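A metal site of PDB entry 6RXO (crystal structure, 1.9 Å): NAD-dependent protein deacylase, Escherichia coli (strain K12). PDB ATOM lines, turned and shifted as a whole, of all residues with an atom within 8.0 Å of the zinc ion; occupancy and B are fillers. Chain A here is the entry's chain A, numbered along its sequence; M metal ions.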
ATOM      1  N   ARG A 129     -17.115  11.806   7.171  1.00  0.00           N
ATOM      2  CA  ARG A 129     -17.402  10.384   7.273  1.00  0.00           C
ATOM      3  C   ARG A 129     -16.124   9.560   7.308  1.00  0.00           C
ATOM      4  O   ARG A 129     -15.169   9.816   6.576  1.00  0.00           O
ATOM      5  CB  ARG A 129     -18.267   9.965   6.073  1.00  0.00           C
ATOM      6  CG  ARG A 129     -18.827   8.557   6.107  1.00  0.00           C
ATOM      7  CD  ARG A 129     -19.299   8.148   4.707  1.00  0.00           C
ATOM      8  NE  ARG A 129     -20.316   9.051   4.176  1.00  0.00           N
ATOM      9  CZ  ARG A 129     -20.796   9.004   2.934  1.00  0.00           C
ATOM     10  NH1 ARG A 129     -20.345   8.089   2.072  1.00  0.00           N
ATOM     11  NH2 ARG A 129     -21.718   9.869   2.536  1.00  0.00           N
ATOM     12  N   CYS A 130     -16.107   8.558   8.185  1.00  0.00           N
ATOM     13  CA  CYS A 130     -14.961   7.664   8.279  1.00  0.00           C
ATOM     14  C   CYS A 130     -14.892   6.792   7.045  1.00  0.00           C
ATOM     15  O   CYS A 130     -15.873   6.170   6.660  1.00  0.00           O
ATOM     16  CB  CYS A 130     -15.046   6.801   9.537  1.00  0.00           C
ATOM     17  SG  CYS A 130     -13.755   5.536   9.622  1.00  0.00           S
ATOM     18  N   SER A 131     -13.714   6.739   6.431  1.00  0.00           N
ATOM     19  CA  SER A 131     -13.525   5.967   5.208  1.00  0.00           C
ATOM     20  C   SER A 131     -13.471   4.465   5.481  1.00  0.00           C
ATOM     21  O   SER A 131     -13.391   3.664   4.553  1.00  0.00           O
ATOM     22  CB  SER A 131     -12.263   6.420   4.493  1.00  0.00           C
ATOM     23  OG  SER A 131     -11.140   6.361   5.361  1.00  0.00           O
ATOM     24  N   GLN A 132     -13.513   4.070   6.755  1.00  0.00           N
ATOM     25  CA  GLN A 132     -13.488   2.658   7.105  1.00  0.00           C
ATOM     26  C   GLN A 132     -14.815   2.128   7.645  1.00  0.00           C
ATOM     27  O   GLN A 132     -15.302   1.093   7.201  1.00  0.00           O
ATOM     28  CB  GLN A 132     -12.396   2.398   8.144  1.00  0.00           C
ATOM     29  CG  GLN A 132     -12.441   0.998   8.758  1.00  0.00           C
ATOM     30  CD  GLN A 132     -12.067  -0.090   7.769  1.00  0.00           C
ATOM     31  OE1 GLN A 132     -12.722  -1.119   7.691  1.00  0.00           O
ATOM     32  NE2 GLN A 132     -10.993   0.136   7.005  1.00  0.00           N
ATOM     33  N   SER A 133     -15.412   2.869   8.569  1.00  0.00           N
ATOM     34  CA  SER A 133     -16.668   2.460   9.172  1.00  0.00           C
ATOM     35  C   SER A 133     -17.893   2.994   8.420  1.00  0.00           C
ATOM     36  O   SER A 133     -18.967   2.399   8.474  1.00  0.00           O
ATOM     37  CB  SER A 133     -16.715   2.902  10.634  1.00  0.00           C
ATOM     38  OG  SER A 133     -16.936   4.296  10.726  1.00  0.00           O
ATOM     39  N   GLY A 134     -17.714   4.126   7.749  1.00  0.00           N
ATOM     40  CA  GLY A 134     -18.806   4.764   7.024  1.00  0.00           C
ATOM     41  C   GLY A 134     -19.627   5.610   7.958  1.00  0.00           C
ATOM     42  O   GLY A 134     -20.674   6.147   7.593  1.00  0.00           O
ATOM     43  N   GLN A 135     -19.129   5.760   9.187  1.00  0.00           N
ATOM     44  CA  GLN A 135     -19.805   6.511  10.240  1.00  0.00           C
ATOM     45  C   GLN A 135     -19.703   8.008   9.993  1.00  0.00           C
ATOM     46  O   GLN A 135     -18.620   8.528   9.719  1.00  0.00           O
ATOM     47  CB  GLN A 135     -19.191   6.145  11.594  1.00  0.00           C
ATOM     48  CG  GLN A 135     -19.908   5.023  12.332  1.00  0.00           C
ATOM     49  CD  GLN A 135     -19.618   5.012  13.814  1.00  0.00           C
ATOM     50  OE1 GLN A 135     -19.680   6.041  14.486  1.00  0.00           O
ATOM     51  NE2 GLN A 135     -19.298   3.833  14.349  1.00  0.00           N
ATOM     52  N   LYS A 148      -8.265  12.380  11.556  1.00  0.00           N
ATOM     53  CA  LYS A 148      -8.717  11.002  11.426  1.00  0.00           C
ATOM     54  C   LYS A 148     -10.050  10.795  12.140  1.00  0.00           C
ATOM     55  O   LYS A 148     -10.552  11.703  12.815  1.00  0.00           O
ATOM     56  CB  LYS A 148      -7.668  10.034  11.968  1.00  0.00           C
ATOM     57  CG  LYS A 148      -6.292  10.146  11.327  1.00  0.00           C
ATOM     58  CD  LYS A 148      -6.335   9.802   9.847  1.00  0.00           C
ATOM     59  CE  LYS A 148      -4.941   9.830   9.233  1.00  0.00           C
ATOM     60  NZ  LYS A 148      -4.238   8.529   9.391  1.00  0.00           N
ATOM     61  N   CYS A 149     -10.610   9.594  12.000  1.00  0.00           N
ATOM     62  CA  CYS A 149     -11.905   9.272  12.599  1.00  0.00           C
ATOM     63  C   CYS A 149     -11.833   9.073  14.112  1.00  0.00           C
ATOM     64  O   CYS A 149     -10.743   8.983  14.683  1.00  0.00           O
ATOM     65  CB  CYS A 149     -12.474   8.002  11.967  1.00  0.00           C
ATOM     66  SG  CYS A 149     -11.653   6.493  12.516  1.00  0.00           S
ATOM     67  N   HIS A 150     -12.991   9.021  14.756  1.00  0.00           N
ATOM     68  CA  HIS A 150     -13.063   8.770  16.189  1.00  0.00           C
ATOM     69  C   HIS A 150     -13.864   7.501  16.465  1.00  0.00           C
ATOM     70  O   HIS A 150     -14.352   7.307  17.576  1.00  0.00           O
ATOM     71  CB  HIS A 150     -13.740   9.924  16.949  1.00  0.00           C
ATOM     72  CG  HIS A 150     -13.236  11.294  16.597  1.00  0.00           C
ATOM     73  ND1 HIS A 150     -13.560  12.403  17.353  1.00  0.00           N
ATOM     74  CD2 HIS A 150     -12.467  11.746  15.586  1.00  0.00           C
ATOM     75  CE1 HIS A 150     -12.999  13.476  16.825  1.00  0.00           C
ATOM     76  NE2 HIS A 150     -12.332  13.106  15.741  1.00  0.00           N
ATOM     77  N   CYS A 151     -14.008   6.649  15.465  1.00  0.00           N
ATOM     78  CA  CYS A 151     -14.834   5.448  15.613  1.00  0.00           C
ATOM     79  C   CYS A 151     -14.063   4.153  15.426  1.00  0.00           C
ATOM     80  O   CYS A 151     -14.597   3.063  15.638  1.00  0.00           O
ATOM     81  CB  CYS A 151     -16.010   5.503  14.634  1.00  0.00           C
ATOM     82  SG  CYS A 151     -15.547   5.884  12.922  1.00  0.00           S
ATOM     83  N   CYS A 152     -12.802   4.269  15.030  1.00  0.00           N
ATOM     84  CA  CYS A 152     -11.984   3.098  14.752  1.00  0.00           C
ATOM     85  C   CYS A 152     -10.776   2.998  15.674  1.00  0.00           C
ATOM     86  O   CYS A 152     -10.148   3.999  15.985  1.00  0.00           O
ATOM     87  CB  CYS A 152     -11.525   3.121  13.295  1.00  0.00           C
ATOM     88  SG  CYS A 152     -12.832   2.816  12.095  1.00  0.00           S
ATOM     89  N   GLN A 153     -10.479   1.781  16.125  1.00  0.00           N
ATOM     90  CA  GLN A 153      -9.265   1.526  16.899  1.00  0.00           C
ATOM     91  C   GLN A 153      -8.043   2.085  16.178  1.00  0.00           C
ATOM     92  O   GLN A 153      -7.182   2.707  16.795  1.00  0.00           O
ATOM     93  CB  GLN A 153      -9.100   0.024  17.145  1.00  0.00           C
ATOM     94  CG  GLN A 153      -7.748  -0.345  17.728  1.00  0.00           C
ATOM     95  CD  GLN A 153      -7.715  -1.753  18.290  1.00  0.00           C
ATOM     96  OE1 GLN A 153      -8.751  -2.403  18.411  1.00  0.00           O
ATOM     97  NE2 GLN A 153      -6.524  -2.225  18.625  1.00  0.00           N
ATOM     98  N   PHE A 154      -7.958   1.818  14.880  1.00  0.00           N
ATOM     99  CA  PHE A 154      -6.905   2.353  14.020  1.00  0.00           C
ATOM    100  C   PHE A 154      -7.460   3.479  13.155  1.00  0.00           C
ATOM    101  O   PHE A 154      -7.956   3.226  12.048  1.00  0.00           O
ATOM    102  CB  PHE A 154      -6.315   1.248  13.129  1.00  0.00           C
ATOM    103  CG  PHE A 154      -5.894   0.026  13.889  1.00  0.00           C
ATOM    104  CD1 PHE A 154      -4.753   0.039  14.681  1.00  0.00           C
ATOM    105  CD2 PHE A 154      -6.622  -1.149  13.792  1.00  0.00           C
ATOM    106  CE1 PHE A 154      -4.352  -1.095  15.368  1.00  0.00           C
ATOM    107  CE2 PHE A 154      -6.229  -2.295  14.477  1.00  0.00           C
ATOM    108  CZ  PHE A 154      -5.094  -2.261  15.275  1.00  0.00           C
ATOM    109  N   PRO A 155      -7.394   4.731  13.653  1.00  0.00           N
ATOM    110  CA  PRO A 155      -7.974   5.922  13.023  1.00  0.00           C
ATOM    111  C   PRO A 155      -7.787   6.001  11.505  1.00  0.00           C
ATOM    112  O   PRO A 155      -6.663   5.970  11.007  1.00  0.00           O
ATOM    113  CB  PRO A 155      -7.243   7.062  13.729  1.00  0.00           C
ATOM    114  CG  PRO A 155      -6.947   6.530  15.078  1.00  0.00           C
ATOM    115  CD  PRO A 155      -6.615   5.078  14.855  1.00  0.00           C
ATOM    116  N   ALA A 156      -8.905   6.095  10.789  1.00  0.00           N
ATOM    117  CA  ALA A 156      -8.918   6.106   9.331  1.00  0.00           C
ATOM    118  C   ALA A 156      -9.059   7.541   8.774  1.00  0.00           C
ATOM    119  O   ALA A 156      -9.529   8.429   9.487  1.00  0.00           O
ATOM    120  CB  ALA A 156     -10.043   5.219   8.810  1.00  0.00           C
ATOM    121  N   PRO A 157      -8.665   7.760   7.509  1.00  0.00           N
ATOM    122  CA  PRO A 157      -8.866   9.061   6.872  1.00  0.00           C
ATOM    123  C   PRO A 157     -10.336   9.460   6.761  1.00  0.00           C
ATOM    124  O   PRO A 157     -11.209   8.600   6.777  1.00  0.00           O
ATOM    125  CB  PRO A 157      -8.259   8.869   5.480  1.00  0.00           C
ATOM    126  CG  PRO A 157      -7.261   7.783   5.648  1.00  0.00           C
ATOM    127  CD  PRO A 157      -7.853   6.857   6.675  1.00  0.00           C
ATOM    128  N   LEU A 158     -10.588  10.762   6.684  1.00  0.00           N
ATOM    129  CA  LEU A 158     -11.949  11.281   6.598  1.00  0.00           C
ATOM    130  C   LEU A 158     -12.293  11.778   5.197  1.00  0.00           C
ATOM    131  O   LEU A 158     -11.426  12.280   4.478  1.00  0.00           O
ATOM    132  CB  LEU A 158     -12.152  12.425   7.602  1.00  0.00           C
ATOM    133  CG  LEU A 158     -11.984  12.082   9.085  1.00  0.00           C
ATOM    134  CD1 LEU A 158     -11.917  13.356   9.911  1.00  0.00           C
ATOM    135  CD2 LEU A 158     -13.111  11.180   9.564  1.00  0.00           C
HETATM  136 ZN    ZN M   1     -13.438   5.124  11.958  1.00  0.00          ZN
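The zinc ion is bound by the side-chain sulfur of Cys 149, the side-chain sulfur of Cys 152, the side-chain sulfur of Cys 130 and the side-chain sulfur of Cys 151.
The zinc ion has four donor atoms within binding distance.
The side-chain sulfur (SG) of Cys 151 lies close to the side-chain hydroxyl (OG) of Ser 133.
The backbone NH (N) of Cys 149 lies within hydrogen-bond range of the backbone carbonyl oxygen (O) of Ala 156 (3.0 Å).
OG of Ser 133 lies close to N of Gln 135, at 3.1 Å.
The backbone NH of Cys 130 lies within hydrogen-bond range of the backbone carbonyl oxygen of Gln 135.
The side-chain sulfur (SG) of Cys 130 lies close to the backbone NH (N) of Gln 132 (3.2 Å).
The backbone NH of Ser 133 lies close to the side-chain sulfur of Cys 130, at 3.3 Å.
OG of Ser 133 touches the zinc ion, 3.8 Å away.
Of the 18 residues printed, 5 come within 4 Å of the zinc ion.
The nearest printed residue that does not touch the zinc ion is Ala 156 (4.6 Å).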
